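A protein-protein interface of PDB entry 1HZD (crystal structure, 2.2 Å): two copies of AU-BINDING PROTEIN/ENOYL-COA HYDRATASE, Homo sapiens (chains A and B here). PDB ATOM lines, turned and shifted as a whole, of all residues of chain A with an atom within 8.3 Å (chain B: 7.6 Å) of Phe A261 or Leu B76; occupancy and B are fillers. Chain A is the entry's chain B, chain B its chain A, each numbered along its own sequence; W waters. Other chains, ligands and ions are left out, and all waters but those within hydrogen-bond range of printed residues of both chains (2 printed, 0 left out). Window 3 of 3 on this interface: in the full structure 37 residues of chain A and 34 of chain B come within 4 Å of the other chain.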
ATOM      1  N   ARG A 254      -4.480   8.534  12.935  1.00  0.00           N
ATOM      2  CA  ARG A 254      -5.183   9.798  13.144  1.00  0.00           C
ATOM      3  C   ARG A 254      -4.227  10.966  12.950  1.00  0.00           C
ATOM      4  O   ARG A 254      -4.583  11.978  12.343  1.00  0.00           O
ATOM      5  CB  ARG A 254      -5.791   9.875  14.551  1.00  0.00           C
ATOM      6  CG  ARG A 254      -6.536  11.190  14.821  1.00  0.00           C
ATOM      7  CD  ARG A 254      -7.185  11.233  16.207  1.00  0.00           C
ATOM      8  NE  ARG A 254      -6.237  11.490  17.296  1.00  0.00           N
ATOM      9  CZ  ARG A 254      -5.738  12.689  17.596  1.00  0.00           C
ATOM     10  NH1 ARG A 254      -6.090  13.755  16.890  1.00  0.00           N
ATOM     11  NH2 ARG A 254      -4.895  12.828  18.610  1.00  0.00           N
ATOM     12  N   LEU A 255      -3.013  10.824  13.480  1.00  0.00           N
ATOM     13  CA  LEU A 255      -2.002  11.870  13.357  1.00  0.00           C
ATOM     14  C   LEU A 255      -1.581  12.024  11.900  1.00  0.00           C
ATOM     15  O   LEU A 255      -1.515  13.138  11.390  1.00  0.00           O
ATOM     16  CB  LEU A 255      -0.785  11.538  14.223  1.00  0.00           C
ATOM     17  CG  LEU A 255      -1.036  11.491  15.734  1.00  0.00           C
ATOM     18  CD1 LEU A 255       0.214  10.967  16.442  1.00  0.00           C
ATOM     19  CD2 LEU A 255      -1.413  12.881  16.242  1.00  0.00           C
ATOM     20  N   GLU A 256      -1.310  10.904  11.233  1.00  0.00           N
ATOM     21  CA  GLU A 256      -0.902  10.931   9.834  1.00  0.00           C
ATOM     22  C   GLU A 256      -1.984  11.592   8.988  1.00  0.00           C
ATOM     23  O   GLU A 256      -1.701  12.162   7.940  1.00  0.00           O
ATOM     24  CB  GLU A 256      -0.643   9.515   9.313  1.00  0.00           C
ATOM     25  CG  GLU A 256       0.721   9.344   8.646  1.00  0.00           C
ATOM     26  CD  GLU A 256       1.878   9.419   9.648  1.00  0.00           C
ATOM     27  OE1 GLU A 256       2.072   8.446  10.415  1.00  0.00           O
ATOM     28  OE2 GLU A 256       2.584  10.453   9.677  1.00  0.00           O
ATOM     29  N   GLY A 257      -3.228  11.508   9.451  1.00  0.00           N
ATOM     30  CA  GLY A 257      -4.325  12.113   8.723  1.00  0.00           C
ATOM     31  C   GLY A 257      -4.246  13.625   8.798  1.00  0.00           C
ATOM     32  O   GLY A 257      -4.437  14.321   7.800  1.00  0.00           O
ATOM     33  N   LEU A 258      -3.963  14.139   9.989  1.00  0.00           N
ATOM     34  CA  LEU A 258      -3.862  15.579  10.183  1.00  0.00           C
ATOM     35  C   LEU A 258      -2.569  16.102   9.567  1.00  0.00           C
ATOM     36  O   LEU A 258      -2.503  17.247   9.120  1.00  0.00           O
ATOM     37  CB  LEU A 258      -3.908  15.922  11.675  1.00  0.00           C
ATOM     38  CG  LEU A 258      -5.209  15.631  12.427  1.00  0.00           C
ATOM     39  CD1 LEU A 258      -5.011  15.878  13.920  1.00  0.00           C
ATOM     40  CD2 LEU A 258      -6.319  16.516  11.893  1.00  0.00           C
ATOM     41  N   LEU A 259      -1.539  15.262   9.548  1.00  0.00           N
ATOM     42  CA  LEU A 259      -0.265  15.661   8.967  1.00  0.00           C
ATOM     43  C   LEU A 259      -0.422  15.688   7.456  1.00  0.00           C
ATOM     44  O   LEU A 259      -0.051  16.662   6.806  1.00  0.00           O
ATOM     45  CB  LEU A 259       0.847  14.681   9.357  1.00  0.00           C
ATOM     46  CG  LEU A 259       2.253  15.016   8.842  1.00  0.00           C
ATOM     47  CD1 LEU A 259       2.655  16.408   9.306  1.00  0.00           C
ATOM     48  CD2 LEU A 259       3.242  13.984   9.348  1.00  0.00           C
ATOM     49  N   ALA A 260      -0.984  14.615   6.907  1.00  0.00           N
ATOM     50  CA  ALA A 260      -1.203  14.511   5.470  1.00  0.00           C
ATOM     51  C   ALA A 260      -2.004  15.704   4.977  1.00  0.00           C
ATOM     52  O   ALA A 260      -1.727  16.244   3.907  1.00  0.00           O
ATOM     53  CB  ALA A 260      -1.933  13.223   5.141  1.00  0.00           C
ATOM     54  N   PHE A 261      -2.997  16.110   5.761  1.00  0.00           N
ATOM     55  CA  PHE A 261      -3.834  17.251   5.409  1.00  0.00           C
ATOM     56  C   PHE A 261      -2.999  18.529   5.377  1.00  0.00           C
ATOM     57  O   PHE A 261      -3.167  19.376   4.494  1.00  0.00           O
ATOM     58  CB  PHE A 261      -4.963  17.415   6.433  1.00  0.00           C
ATOM     59  CG  PHE A 261      -5.813  18.634   6.207  1.00  0.00           C
ATOM     60  CD1 PHE A 261      -6.800  18.640   5.228  1.00  0.00           C
ATOM     61  CD2 PHE A 261      -5.597  19.792   6.943  1.00  0.00           C
ATOM     62  CE1 PHE A 261      -7.556  19.786   4.981  1.00  0.00           C
ATOM     63  CE2 PHE A 261      -6.349  20.947   6.704  1.00  0.00           C
ATOM     64  CZ  PHE A 261      -7.329  20.944   5.722  1.00  0.00           C
ATOM     65  N   LYS A 262      -2.101  18.664   6.349  1.00  0.00           N
ATOM     66  CA  LYS A 262      -1.250  19.846   6.444  1.00  0.00           C
ATOM     67  C   LYS A 262      -0.194  19.887   5.339  1.00  0.00           C
ATOM     68  O   LYS A 262       0.170  20.960   4.857  1.00  0.00           O
ATOM     69  CB  LYS A 262      -0.571  19.891   7.815  1.00  0.00           C
ATOM     70  CG  LYS A 262       0.095  21.222   8.145  1.00  0.00           C
ATOM     71  CD  LYS A 262       0.633  21.225   9.573  1.00  0.00           C
ATOM     72  CE  LYS A 262       1.181  22.590   9.972  1.00  0.00           C
ATOM     73  NZ  LYS A 262       1.608  22.610  11.403  1.00  0.00           N
ATOM     74  N   GLU A 263       0.294  18.720   4.934  1.00  0.00           N
ATOM     75  CA  GLU A 263       1.305  18.659   3.888  1.00  0.00           C
ATOM     76  C   GLU A 263       0.680  18.394   2.517  1.00  0.00           C
ATOM     77  O   GLU A 263       1.355  17.928   1.599  1.00  0.00           O
ATOM     78  CB  GLU A 263       2.336  17.576   4.223  1.00  0.00           C
ATOM     79  CG  GLU A 263       2.939  17.725   5.617  1.00  0.00           C
ATOM     80  CD  GLU A 263       4.158  16.850   5.834  1.00  0.00           C
ATOM     81  OE1 GLU A 263       4.082  15.628   5.572  1.00  0.00           O
ATOM     82  OE2 GLU A 263       5.197  17.386   6.274  1.00  0.00           O
ATOM     83  N   LYS A 264      -0.611  18.705   2.391  1.00  0.00           N
ATOM     84  CA  LYS A 264      -1.362  18.515   1.148  1.00  0.00           C
ATOM     85  C   LYS A 264      -0.843  17.334   0.332  1.00  0.00           C
ATOM     86  O   LYS A 264      -0.242  17.517  -0.729  1.00  0.00           O
ATOM     87  CB  LYS A 264      -1.310  19.792   0.304  1.00  0.00           C
ATOM     88  CG  LYS A 264      -1.878  21.025   1.000  1.00  0.00           C
ATOM     89  CD  LYS A 264      -1.718  22.286   0.151  1.00  0.00           C
ATOM     90  CE  LYS A 264      -2.317  23.508   0.846  1.00  0.00           C
ATOM     91  NZ  LYS A 264      -2.161  24.761   0.045  1.00  0.00           N
ATOM     92  N   ARG A 265      -1.072  16.125   0.841  1.00  0.00           N
ATOM     93  CA  ARG A 265      -0.634  14.896   0.179  1.00  0.00           C
ATOM     94  C   ARG A 265      -1.528  13.737   0.627  1.00  0.00           C
ATOM     95  O   ARG A 265      -2.249  13.852   1.616  1.00  0.00           O
ATOM     96  CB  ARG A 265       0.815  14.572   0.555  1.00  0.00           C
ATOM     97  CG  ARG A 265       0.964  14.025   1.969  1.00  0.00           C
ATOM     98  CD  ARG A 265       2.384  13.580   2.267  1.00  0.00           C
ATOM     99  NE  ARG A 265       2.458  12.737   3.460  1.00  0.00           N
ATOM    100  CZ  ARG A 265       2.126  13.130   4.686  1.00  0.00           C
ATOM    101  NH1 ARG A 265       1.688  14.363   4.900  1.00  0.00           N
ATOM    102  NH2 ARG A 265       2.241  12.291   5.706  1.00  0.00           N
ATOM    103  N   PRO A 266      -1.481  12.605  -0.097  1.00  0.00           N
ATOM    104  CA  PRO A 266      -2.284  11.421   0.230  1.00  0.00           C
ATOM    105  C   PRO A 266      -1.825  10.777   1.541  1.00  0.00           C
ATOM    106  O   PRO A 266      -0.636  10.519   1.730  1.00  0.00           O
ATOM    107  CB  PRO A 266      -2.037  10.491  -0.960  1.00  0.00           C
ATOM    108  CG  PRO A 266      -1.691  11.432  -2.077  1.00  0.00           C
ATOM    109  CD  PRO A 266      -0.796  12.421  -1.389  1.00  0.00           C
ATOM    110  N   PRO A 267      -2.763  10.518   2.463  1.00  0.00           N
ATOM    111  CA  PRO A 267      -2.421   9.897   3.745  1.00  0.00           C
ATOM    112  C   PRO A 267      -1.834   8.496   3.541  1.00  0.00           C
ATOM    113  O   PRO A 267      -2.192   7.797   2.594  1.00  0.00           O
ATOM    114  CB  PRO A 267      -3.767   9.841   4.466  1.00  0.00           C
ATOM    115  CG  PRO A 267      -4.490  11.020   3.921  1.00  0.00           C
ATOM    116  CD  PRO A 267      -4.171  10.949   2.451  1.00  0.00           C
ATOM    117  N   TYR A 269      -1.835   5.351   5.608  1.00  0.00           N
ATOM    118  CA  TYR A 269      -2.336   4.613   6.765  1.00  0.00           C
ATOM    119  C   TYR A 269      -1.848   3.168   6.812  1.00  0.00           C
ATOM    120  O   TYR A 269      -1.694   2.513   5.777  1.00  0.00           O
ATOM    121  CB  TYR A 269      -3.868   4.656   6.769  1.00  0.00           C
ATOM    122  CG  TYR A 269      -4.441   6.062   6.876  1.00  0.00           C
ATOM    123  CD1 TYR A 269      -5.515   6.458   6.087  1.00  0.00           C
ATOM    124  CD2 TYR A 269      -3.917   6.985   7.782  1.00  0.00           C
ATOM    125  CE1 TYR A 269      -6.058   7.741   6.195  1.00  0.00           C
ATOM    126  CE2 TYR A 269      -4.453   8.271   7.896  1.00  0.00           C
ATOM    127  CZ  TYR A 269      -5.524   8.637   7.101  1.00  0.00           C
ATOM    128  OH  TYR A 269      -6.078   9.891   7.226  1.00  0.00           O
ATOM    129  N   GLY B  32     -13.932  30.822   9.206  1.00  0.00           N
ATOM    130  CA  GLY B  32     -13.645  29.442   9.551  1.00  0.00           C
ATOM    131  C   GLY B  32     -14.556  28.461   8.838  1.00  0.00           C
ATOM    132  O   GLY B  32     -14.721  27.325   9.286  1.00  0.00           O
ATOM    133  N   LYS B  33     -15.147  28.889   7.726  1.00  0.00           N
ATOM    134  CA  LYS B  33     -16.047  28.025   6.969  1.00  0.00           C
ATOM    135  C   LYS B  33     -17.131  27.504   7.905  1.00  0.00           C
ATOM    136  O   LYS B  33     -17.580  26.359   7.786  1.00  0.00           O
ATOM    137  CB  LYS B  33     -15.268  26.848   6.381  1.00  0.00           C
ATOM    138  CG  LYS B  33     -14.123  27.254   5.475  1.00  0.00           C
ATOM    139  CD  LYS B  33     -13.281  26.047   5.095  1.00  0.00           C
ATOM    140  CE  LYS B  33     -12.196  26.429   4.101  1.00  0.00           C
ATOM    141  NZ  LYS B  33     -12.781  26.936   2.826  1.00  0.00           N
ATOM    142  N   SER B  35     -16.916  26.460  10.721  1.00  0.00           N
ATOM    143  CA  SER B  35     -16.469  25.251  11.404  1.00  0.00           C
ATOM    144  C   SER B  35     -16.822  25.345  12.889  1.00  0.00           C
ATOM    145  O   SER B  35     -16.998  26.441  13.426  1.00  0.00           O
ATOM    146  CB  SER B  35     -14.954  25.054  11.232  1.00  0.00           C
ATOM    147  OG  SER B  35     -14.209  26.101  11.829  1.00  0.00           O
ATOM    148  N   LEU B  36     -16.934  24.195  13.545  1.00  0.00           N
ATOM    149  CA  LEU B  36     -17.287  24.159  14.959  1.00  0.00           C
ATOM    150  C   LEU B  36     -16.104  24.418  15.886  1.00  0.00           C
ATOM    151  O   LEU B  36     -15.437  23.489  16.343  1.00  0.00           O
ATOM    152  CB  LEU B  36     -17.928  22.816  15.306  1.00  0.00           C
ATOM    153  CG  LEU B  36     -19.169  22.442  14.491  1.00  0.00           C
ATOM    154  CD1 LEU B  36     -19.721  21.128  15.007  1.00  0.00           C
ATOM    155  CD2 LEU B  36     -20.218  23.542  14.593  1.00  0.00           C
ATOM    156  N   ALA B  72     -18.729  23.391   7.799  1.00  0.00           N
ATOM    157  CA  ALA B  72     -17.702  22.457   7.348  1.00  0.00           C
ATOM    158  C   ALA B  72     -17.283  21.428   8.396  1.00  0.00           C
ATOM    159  O   ALA B  72     -16.354  20.652   8.170  1.00  0.00           O
ATOM    160  CB  ALA B  72     -16.479  23.232   6.863  1.00  0.00           C
ATOM    161  N   GLY B  73     -17.965  21.425   9.538  1.00  0.00           N
ATOM    162  CA  GLY B  73     -17.636  20.473  10.581  1.00  0.00           C
ATOM    163  C   GLY B  73     -16.681  21.043  11.607  1.00  0.00           C
ATOM    164  O   GLY B  73     -16.583  22.254  11.767  1.00  0.00           O
ATOM    165  N   ALA B  74     -15.969  20.161  12.301  1.00  0.00           N
ATOM    166  CA  ALA B  74     -15.025  20.573  13.333  1.00  0.00           C
ATOM    167  C   ALA B  74     -13.837  21.323  12.743  1.00  0.00           C
ATOM    168  O   ALA B  74     -13.441  21.093  11.600  1.00  0.00           O
ATOM    169  CB  ALA B  74     -14.542  19.353  14.119  1.00  0.00           C
ATOM    170  N   ASP B  75     -13.277  22.222  13.542  1.00  0.00           N
ATOM    171  CA  ASP B  75     -12.142  23.040  13.134  1.00  0.00           C
ATOM    172  C   ASP B  75     -10.824  22.269  13.168  1.00  0.00           C
ATOM    173  O   ASP B  75     -10.296  21.970  14.235  1.00  0.00           O
ATOM    174  CB  ASP B  75     -12.070  24.268  14.044  1.00  0.00           C
ATOM    175  CG  ASP B  75     -10.929  25.198  13.694  1.00  0.00           C
ATOM    176  OD1 ASP B  75     -10.941  26.337  14.206  1.00  0.00           O
ATOM    177  OD2 ASP B  75     -10.026  24.796  12.926  1.00  0.00           O
ATOM    178  N   LEU B  76     -10.300  21.952  11.989  1.00  0.00           N
ATOM    179  CA  LEU B  76      -9.047  21.218  11.875  1.00  0.00           C
ATOM    180  C   LEU B  76      -7.894  21.916  12.592  1.00  0.00           C
ATOM    181  O   LEU B  76      -7.052  21.269  13.222  1.00  0.00           O
ATOM    182  CB  LEU B  76      -8.683  21.043  10.403  1.00  0.00           C
ATOM    183  CG  LEU B  76      -9.161  19.772   9.709  1.00  0.00           C
ATOM    184  CD1 LEU B  76      -9.373  20.037   8.229  1.00  0.00           C
ATOM    185  CD2 LEU B  76      -8.143  18.661   9.930  1.00  0.00           C
ATOM    186  N   LYS B  77      -7.863  23.240  12.494  1.00  0.00           N
ATOM    187  CA  LYS B  77      -6.803  24.029  13.108  1.00  0.00           C
ATOM    188  C   LYS B  77      -6.718  23.811  14.609  1.00  0.00           C
ATOM    189  O   LYS B  77      -5.667  23.439  15.129  1.00  0.00           O
ATOM    190  CB  LYS B  77      -7.011  25.514  12.798  1.00  0.00           C
ATOM    191  CG  LYS B  77      -5.902  26.420  13.301  1.00  0.00           C
ATOM    192  CD  LYS B  77      -5.921  27.757  12.573  1.00  0.00           C
ATOM    193  CE  LYS B  77      -5.614  27.571  11.094  1.00  0.00           C
ATOM    194  NZ  LYS B  77      -4.270  26.940  10.883  1.00  0.00           N
ATOM    195  N   GLU B  78      -7.826  24.040  15.304  1.00  0.00           N
ATOM    196  CA  GLU B  78      -7.851  23.859  16.748  1.00  0.00           C
ATOM    197  C   GLU B  78      -7.565  22.404  17.133  1.00  0.00           C
ATOM    198  O   GLU B  78      -6.855  22.142  18.102  1.00  0.00           O
ATOM    199  CB  GLU B  78      -9.211  24.277  17.314  1.00  0.00           C
ATOM    200  CG  GLU B  78      -9.681  25.667  16.899  1.00  0.00           C
ATOM    201  CD  GLU B  78     -10.891  26.146  17.701  1.00  0.00           C
ATOM    202  OE1 GLU B  78     -11.894  25.406  17.796  1.00  0.00           O
ATOM    203  OE2 GLU B  78     -10.841  27.271  18.239  1.00  0.00           O
ATOM    204  N   ARG B  79      -8.101  21.460  16.361  1.00  0.00           N
ATOM    205  CA  ARG B  79      -7.916  20.038  16.653  1.00  0.00           C
ATOM    206  C   ARG B  79      -6.468  19.578  16.680  1.00  0.00           C
ATOM    207  O   ARG B  79      -6.091  18.742  17.507  1.00  0.00           O
ATOM    208  CB  ARG B  79      -8.670  19.167  15.645  1.00  0.00           C
ATOM    209  CG  ARG B  79      -8.588  17.679  15.977  1.00  0.00           C
ATOM    210  CD  ARG B  79      -9.219  17.428  17.346  1.00  0.00           C
ATOM    211  NE  ARG B  79     -10.603  17.890  17.340  1.00  0.00           N
ATOM    212  CZ  ARG B  79     -11.617  17.195  16.834  1.00  0.00           C
ATOM    213  NH1 ARG B  79     -11.406  15.995  16.310  1.00  0.00           N
ATOM    214  NH2 ARG B  79     -12.835  17.723  16.808  1.00  0.00           N
ATOM    215  N   ALA B  80      -5.664  20.109  15.764  1.00  0.00           N
ATOM    216  CA  ALA B  80      -4.257  19.741  15.675  1.00  0.00           C
ATOM    217  C   ALA B  80      -3.449  20.314  16.839  1.00  0.00           C
ATOM    218  O   ALA B  80      -2.289  19.953  17.040  1.00  0.00           O
ATOM    219  CB  ALA B  80      -3.687  20.220  14.350  1.00  0.00           C
ATOM    220  N   LYS B  81      -4.071  21.206  17.604  1.00  0.00           N
ATOM    221  CA  LYS B  81      -3.424  21.835  18.751  1.00  0.00           C
ATOM    222  C   LYS B  81      -3.974  21.238  20.043  1.00  0.00           C
ATOM    223  O   LYS B  81      -3.728  21.751  21.139  1.00  0.00           O
ATOM    224  CB  LYS B  81      -3.684  23.344  18.724  1.00  0.00           C
ATOM    225  CG  LYS B  81      -3.194  24.025  17.452  1.00  0.00           C
ATOM    226  CD  LYS B  81      -3.894  25.356  17.200  1.00  0.00           C
ATOM    227  CE  LYS B  81      -3.663  26.354  18.323  1.00  0.00           C
ATOM    228  NZ  LYS B  81      -4.341  27.662  18.050  1.00  0.00           N
ATOM    229  N   MET B  82      -4.722  20.149  19.904  1.00  0.00           N
ATOM    230  CA  MET B  82      -5.318  19.479  21.051  1.00  0.00           C
ATOM    231  C   MET B  82      -4.584  18.191  21.401  1.00  0.00           C
ATOM    232  O   MET B  82      -4.193  17.430  20.514  1.00  0.00           O
ATOM    233  CB  MET B  82      -6.788  19.152  20.766  1.00  0.00           C
ATOM    234  CG  MET B  82      -7.726  20.349  20.817  1.00  0.00           C
ATOM    235  SD  MET B  82      -9.466  19.876  20.701  1.00  0.00           S
ATOM    236  CE  MET B  82      -9.952  20.667  19.172  1.00  0.00           C
ATOM    237  N   LEU B 145      -9.686  10.670   7.218  1.00  0.00           N
ATOM    238  CA  LEU B 145      -8.794  11.265   8.201  1.00  0.00           C
ATOM    239  C   LEU B 145      -8.485  10.284   9.327  1.00  0.00           C
ATOM    240  O   LEU B 145      -7.870  10.645  10.331  1.00  0.00           O
ATOM    241  CB  LEU B 145      -9.421  12.532   8.769  1.00  0.00           C
ATOM    242  CG  LEU B 145      -9.389  13.735   7.832  1.00  0.00           C
ATOM    243  CD1 LEU B 145     -10.274  14.840   8.384  1.00  0.00           C
ATOM    244  CD2 LEU B 145      -7.951  14.206   7.677  1.00  0.00           C
ATOM    245  N   ILE B 147     -10.597   8.818  11.334  1.00  0.00           N
ATOM    246  CA  ILE B 147     -11.462   8.991  12.493  1.00  0.00           C
ATOM    247  C   ILE B 147     -12.849   8.609  11.985  1.00  0.00           C
ATOM    248  O   ILE B 147     -12.995   8.198  10.838  1.00  0.00           O
ATOM    249  CB  ILE B 147     -11.469  10.443  12.995  1.00  0.00           C
ATOM    250  CG1 ILE B 147     -11.731  11.392  11.823  1.00  0.00           C
ATOM    251  CG2 ILE B 147     -10.146  10.753  13.697  1.00  0.00           C
ATOM    252  CD1 ILE B 147     -11.799  12.838  12.210  1.00  0.00           C
HETATM  253  O   HOH W   1      -7.247  12.964  11.564  1.00  0.00           O
HETATM  254  O   HOH W   2      -9.377  14.016  16.155  1.00  0.00           O
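O of Leu B145 touches CA of Arg A254, 3.98 Å away. Ile B147 touches Arg A254 (CG2 to CG, 3.8 Å). Leu B145 touches Gly A257 (CD2 to O, 3.5 Å). Leu B76 touches Leu A258. Leu B76 touches Phe A261. Leu B145 touches Tyr A269 (CA to OH, 3.2 Å).
Of the printed residues of chain B, Arg A254 touches Leu B145 and Ile B147. Of the printed residues of chain B, Gly A257 touches Leu B145 (3.5 Å). No residue of chain B comes within 4 Å of Ala A260. Of chain B, only Leu B76 comes within 4 Å of Phe A261. Printed residues of chain B within 4 Å of Tyr A269: Leu B145. Of chain A, only Leu A258 (3.4 Å) and Phe A261 (3.4 Å) come within 4 Å of Leu B76. Printed residues of chain A within 4 Å of Ile B147: Arg A254 (3.8 Å). The nearest residue of chain B that does not touch Phe A261 is Leu B145 (4.6 Å). The nearest residue of chain A that does not touch Leu B76 is Gly A257 (6.1 Å).
Of the 15 printed residues of chain A, 5 touch a printed residue of chain B. Hydrophobic or aromatic side chains of chain A that line the printed part of chain B: Leu A258, Phe A261 and Tyr A269. Along chain A the printed residues that touch a printed residue of chain B span positions 254 to 269. Among the printed residues, no Asp or Glu carboxylate lies within 4 Å of a Lys or Arg side-chain nitrogen of the other chain.
No position is printed for both chains. Of the 6 pairs that touch across the chains among the printed residues, none has its exchanged pair printed and touching as well.
Water W1 bridges the backbone carbonyl oxygen (O) of Leu B145 (2.7 Å) and the backbone carbonyl oxygen (O) of Arg A254 (2.9 Å). Water W2 bridges NH1 of Arg B79 (2.8 Å) and NH1 of Arg A254 (3.4 Å).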
